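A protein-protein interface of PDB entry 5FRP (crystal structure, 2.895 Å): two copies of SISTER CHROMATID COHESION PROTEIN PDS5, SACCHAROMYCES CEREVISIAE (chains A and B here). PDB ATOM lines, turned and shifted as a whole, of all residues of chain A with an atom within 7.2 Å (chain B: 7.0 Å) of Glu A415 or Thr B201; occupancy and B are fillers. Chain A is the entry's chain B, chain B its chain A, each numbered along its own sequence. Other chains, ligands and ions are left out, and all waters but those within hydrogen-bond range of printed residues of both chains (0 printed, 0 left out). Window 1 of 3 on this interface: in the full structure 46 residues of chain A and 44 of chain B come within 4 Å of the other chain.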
ATOM      1  N   PRO A 374      -5.273  24.666  -4.617  1.00  0.00           N
ATOM      2  CA  PRO A 374      -6.537  25.381  -4.396  1.00  0.00           C
ATOM      3  C   PRO A 374      -6.341  26.860  -4.081  1.00  0.00           C
ATOM      4  O   PRO A 374      -7.269  27.656  -4.230  1.00  0.00           O
ATOM      5  CB  PRO A 374      -7.149  24.646  -3.201  1.00  0.00           C
ATOM      6  CG  PRO A 374      -5.986  24.076  -2.474  1.00  0.00           C
ATOM      7  CD  PRO A 374      -4.973  23.727  -3.523  1.00  0.00           C
ATOM      8  N   ARG A 375      -5.140  27.216  -3.643  1.00  0.00           N
ATOM      9  CA  ARG A 375      -4.816  28.598  -3.319  1.00  0.00           C
ATOM     10  C   ARG A 375      -4.961  29.503  -4.539  1.00  0.00           C
ATOM     11  O   ARG A 375      -5.657  30.522  -4.488  1.00  0.00           O
ATOM     12  CB  ARG A 375      -3.395  28.691  -2.770  1.00  0.00           C
ATOM     13  CG  ARG A 375      -3.279  28.206  -1.340  1.00  0.00           C
ATOM     14  CD  ARG A 375      -1.853  27.840  -0.994  1.00  0.00           C
ATOM     15  NE  ARG A 375      -0.951  28.979  -1.128  1.00  0.00           N
ATOM     16  CZ  ARG A 375       0.350  28.879  -1.385  1.00  0.00           C
ATOM     17  NH1 ARG A 375       0.917  27.688  -1.549  1.00  0.00           N
ATOM     18  NH2 ARG A 375       1.085  29.976  -1.488  1.00  0.00           N
ATOM     19  N   ARG A 378      -8.590  29.798  -5.512  1.00  0.00           N
ATOM     20  CA  ARG A 378      -9.273  30.749  -4.643  1.00  0.00           C
ATOM     21  C   ARG A 378      -8.938  32.175  -5.068  1.00  0.00           C
ATOM     22  O   ARG A 378      -9.835  32.990  -5.316  1.00  0.00           O
ATOM     23  CB  ARG A 378      -8.873  30.529  -3.182  1.00  0.00           C
ATOM     24  CG  ARG A 378      -9.593  31.454  -2.206  1.00  0.00           C
ATOM     25  CD  ARG A 378      -9.034  31.374  -0.795  1.00  0.00           C
ATOM     26  NE  ARG A 378      -7.616  31.727  -0.749  1.00  0.00           N
ATOM     27  CZ  ARG A 378      -6.605  30.870  -0.639  1.00  0.00           C
ATOM     28  NH1 ARG A 378      -6.816  29.562  -0.548  1.00  0.00           N
ATOM     29  NH2 ARG A 378      -5.361  31.331  -0.612  1.00  0.00           N
ATOM     30  N   VAL A 381     -10.796  33.056  -8.246  1.00  0.00           N
ATOM     31  CA  VAL A 381     -12.204  33.412  -8.118  1.00  0.00           C
ATOM     32  C   VAL A 381     -12.336  34.750  -7.391  1.00  0.00           C
ATOM     33  O   VAL A 381     -13.287  35.494  -7.629  1.00  0.00           O
ATOM     34  CB  VAL A 381     -13.038  32.321  -7.392  1.00  0.00           C
ATOM     35  CG1 VAL A 381     -12.774  30.951  -8.003  1.00  0.00           C
ATOM     36  CG2 VAL A 381     -12.768  32.305  -5.897  1.00  0.00           C
ATOM     37  N   LYS A 412     -14.824  19.228  -4.380  1.00  0.00           N
ATOM     38  CA  LYS A 412     -14.625  18.640  -3.063  1.00  0.00           C
ATOM     39  C   LYS A 412     -14.028  19.649  -2.086  1.00  0.00           C
ATOM     40  O   LYS A 412     -14.519  19.796  -0.966  1.00  0.00           O
ATOM     41  CB  LYS A 412     -13.712  17.415  -3.153  1.00  0.00           C
ATOM     42  CG  LYS A 412     -14.333  16.214  -3.844  1.00  0.00           C
ATOM     43  CD  LYS A 412     -15.269  15.448  -2.925  1.00  0.00           C
ATOM     44  CE  LYS A 412     -15.886  14.244  -3.619  1.00  0.00           C
ATOM     45  NZ  LYS A 412     -14.911  13.139  -3.828  1.00  0.00           N
ATOM     46  N   HIS A 413     -12.967  20.333  -2.508  1.00  0.00           N
ATOM     47  CA  HIS A 413     -12.305  21.327  -1.664  1.00  0.00           C
ATOM     48  C   HIS A 413     -13.323  22.333  -1.131  1.00  0.00           C
ATOM     49  O   HIS A 413     -14.120  22.883  -1.891  1.00  0.00           O
ATOM     50  CB  HIS A 413     -11.200  22.045  -2.438  1.00  0.00           C
ATOM     51  CG  HIS A 413     -10.235  22.781  -1.561  1.00  0.00           C
ATOM     52  ND1 HIS A 413     -10.535  23.988  -0.967  1.00  0.00           N
ATOM     53  CD2 HIS A 413      -8.971  22.478  -1.183  1.00  0.00           C
ATOM     54  CE1 HIS A 413      -9.497  24.395  -0.257  1.00  0.00           C
ATOM     55  NE2 HIS A 413      -8.533  23.498  -0.373  1.00  0.00           N
ATOM     56  N   LYS A 414     -13.284  22.556   0.177  1.00  0.00           N
ATOM     57  CA  LYS A 414     -14.293  23.339   0.880  1.00  0.00           C
ATOM     58  C   LYS A 414     -14.058  24.845   0.729  1.00  0.00           C
ATOM     59  O   LYS A 414     -14.962  25.589   0.324  1.00  0.00           O
ATOM     60  CB  LYS A 414     -14.297  22.950   2.360  1.00  0.00           C
ATOM     61  CG  LYS A 414     -15.452  23.521   3.157  1.00  0.00           C
ATOM     62  CD  LYS A 414     -15.164  23.523   4.652  1.00  0.00           C
ATOM     63  CE  LYS A 414     -14.151  24.592   5.050  1.00  0.00           C
ATOM     64  NZ  LYS A 414     -13.605  24.329   6.406  1.00  0.00           N
ATOM     65  N   GLU A 415     -12.847  25.284   1.054  1.00  0.00           N
ATOM     66  CA  GLU A 415     -12.519  26.706   1.075  1.00  0.00           C
ATOM     67  C   GLU A 415     -12.787  27.342  -0.288  1.00  0.00           C
ATOM     68  O   GLU A 415     -13.192  28.501  -0.371  1.00  0.00           O
ATOM     69  CB  GLU A 415     -11.058  26.908   1.479  1.00  0.00           C
ATOM     70  CG  GLU A 415     -10.822  28.179   2.275  1.00  0.00           C
ATOM     71  CD  GLU A 415      -9.382  28.339   2.718  1.00  0.00           C
ATOM     72  OE1 GLU A 415      -8.590  27.388   2.548  1.00  0.00           O
ATOM     73  OE2 GLU A 415      -9.047  29.420   3.246  1.00  0.00           O
ATOM     74  N   VAL A 416     -12.557  26.577  -1.351  1.00  0.00           N
ATOM     75  CA  VAL A 416     -12.873  27.015  -2.705  1.00  0.00           C
ATOM     76  C   VAL A 416     -14.387  27.077  -2.860  1.00  0.00           C
ATOM     77  O   VAL A 416     -14.935  28.109  -3.254  1.00  0.00           O
ATOM     78  CB  VAL A 416     -12.255  26.071  -3.761  1.00  0.00           C
ATOM     79  CG1 VAL A 416     -12.853  26.327  -5.145  1.00  0.00           C
ATOM     80  CG2 VAL A 416     -10.744  26.236  -3.794  1.00  0.00           C
ATOM     81  N   ARG A 417     -15.048  25.969  -2.540  1.00  0.00           N
ATOM     82  CA  ARG A 417     -16.491  25.842  -2.699  1.00  0.00           C
ATOM     83  C   ARG A 417     -17.204  27.052  -2.120  1.00  0.00           C
ATOM     84  O   ARG A 417     -18.009  27.695  -2.794  1.00  0.00           O
ATOM     85  CB  ARG A 417     -16.984  24.573  -1.998  1.00  0.00           C
ATOM     86  CG  ARG A 417     -18.462  24.284  -2.202  1.00  0.00           C
ATOM     87  CD  ARG A 417     -18.961  23.207  -1.250  1.00  0.00           C
ATOM     88  NE  ARG A 417     -18.037  22.075  -1.175  1.00  0.00           N
ATOM     89  CZ  ARG A 417     -17.628  21.496  -0.047  1.00  0.00           C
ATOM     90  NH1 ARG A 417     -18.053  21.928   1.136  1.00  0.00           N
ATOM     91  NH2 ARG A 417     -16.786  20.473  -0.104  1.00  0.00           N
ATOM     92  N   GLU A 418     -16.887  27.359  -0.871  1.00  0.00           N
ATOM     93  CA  GLU A 418     -17.570  28.417  -0.139  1.00  0.00           C
ATOM     94  C   GLU A 418     -17.449  29.776  -0.841  1.00  0.00           C
ATOM     95  O   GLU A 418     -18.464  30.397  -1.204  1.00  0.00           O
ATOM     96  CB  GLU A 418     -17.016  28.500   1.283  1.00  0.00           C
ATOM     97  CG  GLU A 418     -17.211  27.188   2.044  1.00  0.00           C
ATOM     98  CD  GLU A 418     -16.272  27.015   3.221  1.00  0.00           C
ATOM     99  OE1 GLU A 418     -15.240  27.718   3.287  1.00  0.00           O
ATOM    100  OE2 GLU A 418     -16.590  26.188   4.102  1.00  0.00           O
ATOM    101  N   LEU A 419     -16.211  30.223  -1.035  1.00  0.00           N
ATOM    102  CA  LEU A 419     -15.945  31.484  -1.718  1.00  0.00           C
ATOM    103  C   LEU A 419     -16.622  31.505  -3.076  1.00  0.00           C
ATOM    104  O   LEU A 419     -17.189  32.519  -3.477  1.00  0.00           O
ATOM    105  CB  LEU A 419     -14.440  31.702  -1.874  1.00  0.00           C
ATOM    106  CG  LEU A 419     -14.016  32.997  -2.574  1.00  0.00           C
ATOM    107  CD1 LEU A 419     -14.475  34.223  -1.796  1.00  0.00           C
ATOM    108  CD2 LEU A 419     -12.511  33.013  -2.753  1.00  0.00           C
ATOM    109  N   CYS A 420     -16.542  30.384  -3.780  1.00  0.00           N
ATOM    110  CA  CYS A 420     -17.182  30.246  -5.079  1.00  0.00           C
ATOM    111  C   CYS A 420     -18.674  30.569  -4.970  1.00  0.00           C
ATOM    112  O   CYS A 420     -19.177  31.476  -5.652  1.00  0.00           O
ATOM    113  CB  CYS A 420     -16.975  28.828  -5.606  1.00  0.00           C
ATOM    114  SG  CYS A 420     -17.567  28.599  -7.270  1.00  0.00           S
ATOM    115  N   PRO B 161      -8.677  19.414   3.766  1.00  0.00           N
ATOM    116  CA  PRO B 161      -9.597  20.413   3.221  1.00  0.00           C
ATOM    117  C   PRO B 161     -10.769  19.809   2.440  1.00  0.00           C
ATOM    118  O   PRO B 161     -11.856  20.386   2.395  1.00  0.00           O
ATOM    119  CB  PRO B 161      -8.705  21.232   2.284  1.00  0.00           C
ATOM    120  CG  PRO B 161      -7.340  21.114   2.870  1.00  0.00           C
ATOM    121  CD  PRO B 161      -7.266  19.755   3.504  1.00  0.00           C
ATOM    122  N   LEU B 194       0.784  21.055  10.548  1.00  0.00           N
ATOM    123  CA  LEU B 194      -0.647  20.915  10.308  1.00  0.00           C
ATOM    124  C   LEU B 194      -1.474  21.719  11.315  1.00  0.00           C
ATOM    125  O   LEU B 194      -2.315  22.526  10.925  1.00  0.00           O
ATOM    126  CB  LEU B 194      -1.046  19.439  10.351  1.00  0.00           C
ATOM    127  CG  LEU B 194      -2.211  19.006   9.456  1.00  0.00           C
ATOM    128  CD1 LEU B 194      -1.937  19.313   7.993  1.00  0.00           C
ATOM    129  CD2 LEU B 194      -2.472  17.532   9.645  1.00  0.00           C
ATOM    130  N   PHE B 196      -0.613  24.112  13.462  1.00  0.00           N
ATOM    131  CA  PHE B 196      -0.309  25.532  13.621  1.00  0.00           C
ATOM    132  C   PHE B 196      -0.571  26.386  12.377  1.00  0.00           C
ATOM    133  O   PHE B 196      -1.011  27.529  12.496  1.00  0.00           O
ATOM    134  CB  PHE B 196       1.147  25.710  14.053  1.00  0.00           C
ATOM    135  CG  PHE B 196       1.407  25.266  15.465  1.00  0.00           C
ATOM    136  CD1 PHE B 196       0.675  25.794  16.516  1.00  0.00           C
ATOM    137  CD2 PHE B 196       2.371  24.313  15.738  1.00  0.00           C
ATOM    138  CE1 PHE B 196       0.907  25.387  17.811  1.00  0.00           C
ATOM    139  CE2 PHE B 196       2.607  23.901  17.032  1.00  0.00           C
ATOM    140  CZ  PHE B 196       1.873  24.437  18.072  1.00  0.00           C
ATOM    141  N   ASN B 197      -0.310  25.849  11.187  1.00  0.00           N
ATOM    142  CA  ASN B 197      -0.530  26.627   9.967  1.00  0.00           C
ATOM    143  C   ASN B 197      -1.968  27.125   9.830  1.00  0.00           C
ATOM    144  O   ASN B 197      -2.214  28.129   9.164  1.00  0.00           O
ATOM    145  CB  ASN B 197      -0.160  25.808   8.730  1.00  0.00           C
ATOM    146  CG  ASN B 197       1.273  26.031   8.294  1.00  0.00           C
ATOM    147  OD1 ASN B 197       1.754  27.164   8.259  1.00  0.00           O
ATOM    148  ND2 ASN B 197       1.969  24.950   7.966  1.00  0.00           N
ATOM    149  N   LYS B 198      -2.911  26.434  10.463  1.00  0.00           N
ATOM    150  CA  LYS B 198      -4.317  26.814  10.368  1.00  0.00           C
ATOM    151  C   LYS B 198      -4.560  28.212  10.929  1.00  0.00           C
ATOM    152  O   LYS B 198      -5.501  28.890  10.519  1.00  0.00           O
ATOM    153  CB  LYS B 198      -5.206  25.804  11.099  1.00  0.00           C
ATOM    154  CG  LYS B 198      -5.746  24.682  10.220  1.00  0.00           C
ATOM    155  CD  LYS B 198      -6.726  25.196   9.167  1.00  0.00           C
ATOM    156  CE  LYS B 198      -7.279  24.056   8.322  1.00  0.00           C
ATOM    157  NZ  LYS B 198      -8.040  24.568   7.146  1.00  0.00           N
ATOM    158  N   PHE B 199      -3.721  28.637  11.869  1.00  0.00           N
ATOM    159  CA  PHE B 199      -3.790  30.001  12.380  1.00  0.00           C
ATOM    160  C   PHE B 199      -3.401  30.983  11.281  1.00  0.00           C
ATOM    161  O   PHE B 199      -3.944  32.087  11.206  1.00  0.00           O
ATOM    162  CB  PHE B 199      -2.879  30.174  13.597  1.00  0.00           C
ATOM    163  CG  PHE B 199      -3.429  29.558  14.851  1.00  0.00           C
ATOM    164  CD1 PHE B 199      -4.511  30.129  15.499  1.00  0.00           C
ATOM    165  CD2 PHE B 199      -2.865  28.412  15.379  1.00  0.00           C
ATOM    166  CE1 PHE B 199      -5.020  29.566  16.653  1.00  0.00           C
ATOM    167  CE2 PHE B 199      -3.369  27.842  16.531  1.00  0.00           C
ATOM    168  CZ  PHE B 199      -4.449  28.421  17.169  1.00  0.00           C
ATOM    169  N   LEU B 200      -2.456  30.576  10.438  1.00  0.00           N
ATOM    170  CA  LEU B 200      -2.011  31.403   9.322  1.00  0.00           C
ATOM    171  C   LEU B 200      -3.008  31.383   8.167  1.00  0.00           C
ATOM    172  O   LEU B 200      -3.308  32.425   7.584  1.00  0.00           O
ATOM    173  CB  LEU B 200      -0.644  30.934   8.815  1.00  0.00           C
ATOM    174  CG  LEU B 200       0.530  31.018   9.790  1.00  0.00           C
ATOM    175  CD1 LEU B 200       1.795  30.522   9.110  1.00  0.00           C
ATOM    176  CD2 LEU B 200       0.718  32.436  10.303  1.00  0.00           C
ATOM    177  N   THR B 201      -3.517  30.198   7.845  1.00  0.00           N
ATOM    178  CA  THR B 201      -4.263  29.995   6.605  1.00  0.00           C
ATOM    179  C   THR B 201      -5.760  30.253   6.754  1.00  0.00           C
ATOM    180  O   THR B 201      -6.493  30.261   5.764  1.00  0.00           O
ATOM    181  CB  THR B 201      -4.070  28.568   6.066  1.00  0.00           C
ATOM    182  OG1 THR B 201      -4.592  27.624   7.011  1.00  0.00           O
ATOM    183  CG2 THR B 201      -2.596  28.275   5.813  1.00  0.00           C
ATOM    184  N   TYR B 202      -6.211  30.464   7.986  1.00  0.00           N
ATOM    185  CA  TYR B 202      -7.610  30.787   8.239  1.00  0.00           C
ATOM    186  C   TYR B 202      -7.708  31.955   9.202  1.00  0.00           C
ATOM    187  O   TYR B 202      -7.551  31.789  10.410  1.00  0.00           O
ATOM    188  CB  TYR B 202      -8.352  29.571   8.803  1.00  0.00           C
ATOM    189  CG  TYR B 202      -9.777  29.870   9.222  1.00  0.00           C
ATOM    190  CD1 TYR B 202     -10.066  30.306  10.507  1.00  0.00           C
ATOM    191  CD2 TYR B 202     -10.829  29.715   8.329  1.00  0.00           C
ATOM    192  CE1 TYR B 202     -11.363  30.581  10.894  1.00  0.00           C
ATOM    193  CE2 TYR B 202     -12.131  29.986   8.707  1.00  0.00           C
ATOM    194  CZ  TYR B 202     -12.390  30.418   9.991  1.00  0.00           C
ATOM    195  OH  TYR B 202     -13.683  30.690  10.374  1.00  0.00           O
ATOM    196  N   ASN B 203      -7.963  33.138   8.656  1.00  0.00           N
ATOM    197  CA  ASN B 203      -8.160  34.326   9.468  1.00  0.00           C
ATOM    198  C   ASN B 203      -9.621  34.746   9.374  1.00  0.00           C
ATOM    199  O   ASN B 203     -10.099  35.088   8.292  1.00  0.00           O
ATOM    200  CB  ASN B 203      -7.238  35.452   9.001  1.00  0.00           C
ATOM    201  CG  ASN B 203      -6.868  36.408  10.118  1.00  0.00           C
ATOM    202  OD1 ASN B 203      -7.535  36.465  11.152  1.00  0.00           O
ATOM    203  ND2 ASN B 203      -5.804  37.173   9.912  1.00  0.00           N
ATOM    204  N   GLU B 206     -12.012  38.369   7.695  1.00  0.00           N
ATOM    205  CA  GLU B 206     -11.307  38.828   6.501  1.00  0.00           C
ATOM    206  C   GLU B 206     -12.293  39.259   5.420  1.00  0.00           C
ATOM    207  O   GLU B 206     -12.025  40.202   4.675  1.00  0.00           O
ATOM    208  CB  GLU B 206     -10.389  37.719   5.968  1.00  0.00           C
ATOM    209  CG  GLU B 206      -9.895  37.955   4.542  1.00  0.00           C
ATOM    210  CD  GLU B 206      -8.872  36.930   4.088  1.00  0.00           C
ATOM    211  OE1 GLU B 206      -8.270  36.272   4.963  1.00  0.00           O
ATOM    212  OE2 GLU B 206      -8.668  36.781   2.863  1.00  0.00           O
ATOM    213  N   THR B 214     -19.777  30.135   7.773  1.00  0.00           N
ATOM    214  CA  THR B 214     -19.015  29.140   7.033  1.00  0.00           C
ATOM    215  C   THR B 214     -18.220  28.196   7.944  1.00  0.00           C
ATOM    216  O   THR B 214     -18.366  26.978   7.850  1.00  0.00           O
ATOM    217  CB  THR B 214     -18.059  29.842   6.059  1.00  0.00           C
ATOM    218  OG1 THR B 214     -18.801  30.789   5.280  1.00  0.00           O
ATOM    219  CG2 THR B 214     -17.411  28.861   5.139  1.00  0.00           C
ATOM    220  N   ASP B 216     -14.738  26.511  10.056  1.00  0.00           N
ATOM    221  CA  ASP B 216     -13.676  25.614   9.601  1.00  0.00           C
ATOM    222  C   ASP B 216     -13.304  24.617  10.699  1.00  0.00           C
ATOM    223  O   ASP B 216     -13.029  25.007  11.834  1.00  0.00           O
ATOM    224  CB  ASP B 216     -12.456  26.427   9.171  1.00  0.00           C
ATOM    225  CG  ASP B 216     -11.333  25.572   8.622  1.00  0.00           C
ATOM    226  OD1 ASP B 216     -11.605  24.530   7.989  1.00  0.00           O
ATOM    227  OD2 ASP B 216     -10.159  25.941   8.828  1.00  0.00           O
ATOM    228  N   LYS B 263       7.184  34.574   9.473  1.00  0.00           N
ATOM    229  CA  LYS B 263       5.940  33.807   9.495  1.00  0.00           C
ATOM    230  C   LYS B 263       5.634  33.314  10.904  1.00  0.00           C
ATOM    231  O   LYS B 263       4.494  33.415  11.379  1.00  0.00           O
ATOM    232  CB  LYS B 263       6.025  32.614   8.540  1.00  0.00           C
ATOM    233  CG  LYS B 263       5.156  32.757   7.301  1.00  0.00           C
ATOM    234  CD  LYS B 263       5.019  31.424   6.581  1.00  0.00           C
ATOM    235  CE  LYS B 263       4.054  31.525   5.411  1.00  0.00           C
ATOM    236  NZ  LYS B 263       3.589  30.175   4.982  1.00  0.00           N
ATOM    237  N   LYS B 266       4.070  35.877  12.820  1.00  0.00           N
ATOM    238  CA  LYS B 266       2.641  36.004  12.551  1.00  0.00           C
ATOM    239  C   LYS B 266       1.862  34.943  13.320  1.00  0.00           C
ATOM    240  O   LYS B 266       0.830  35.240  13.931  1.00  0.00           O
ATOM    241  CB  LYS B 266       2.359  35.881  11.051  1.00  0.00           C
ATOM    242  CG  LYS B 266       1.003  36.438  10.642  1.00  0.00           C
ATOM    243  CD  LYS B 266       0.824  36.427   9.133  1.00  0.00           C
ATOM    244  CE  LYS B 266      -0.544  36.970   8.745  1.00  0.00           C
ATOM    245  NZ  LYS B 266      -0.892  36.622   7.338  1.00  0.00           N
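Hydrophobic or aromatic side chains of chain A within 4 Å of the printed part of chain B: His A413. Of the 15 printed residues of chain B, 4 touch a printed residue of chain A. Printed residues of chain B that touch a printed residue of chain A: Pro B161, Thr B201, Thr B214 and Asp B216. Hydrophobic or aromatic side chains of chain B within 4 Å of the printed part of chain A: Pro B161. Among the printed residues, Asp or Glu carboxylates within 4 Å of a Lys or Arg side-chain nitrogen of the other chain: Lys A414 with Asp B216 (2.6 Å).
The backbone carbonyl oxygen (O) of Asn B197 lies within hydrogen-bond range of the side-chain hydroxyl (OG1) of Thr B201 (3.2 Å). The side-chain carboxylate of Asp B216 is in salt-bridge range of the side-chain amino group of Lys B198, at 3.0 Å. A ring nitrogen (ND1) of His A413 lies within hydrogen-bond range of the backbone NH (N) of Val A416 (3.3 Å). A ring nitrogen (ND1) of His A413 lies within hydrogen-bond range of the backbone NH (N) of Glu A415.
No position is printed for both chains. Of the 5 pairs that touch across the chains among the printed residues, none has its exchanged pair printed and touching as well.
Among the printed residues, merely in contact across the chains: Glu A418 with Thr B214 (2.9 Å), His A413 with Pro B161 (3.5 Å) and Glu A415 with Thr B201 (3.7 Å).
Glu A415 touches just one residue of chain B: Thr B201. Of chain A, only Glu A415 comes within 4 Å of Thr B201. Of the printed residues of chain B, His A413 touches Pro B161 (3.5 Å). Printed residues of chain B within 4 Å of Lys A414: Pro B161 (3.4 Å) and Asp B216 (2.6 Å). Arg A375 touches none of the printed residues of chain B. The nearest residue of chain A that does not touch Thr B201 is Arg A378 (6.4 Å). The nearest printed residue of chain A that does not touch Pro B161 is Lys A412 (4.3 Å).
NZ of Lys A414 is in salt-bridge range of OD1 of Asp B216. O of Pro B161 sits at hydrogen-bond distance from N of Lys A414.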
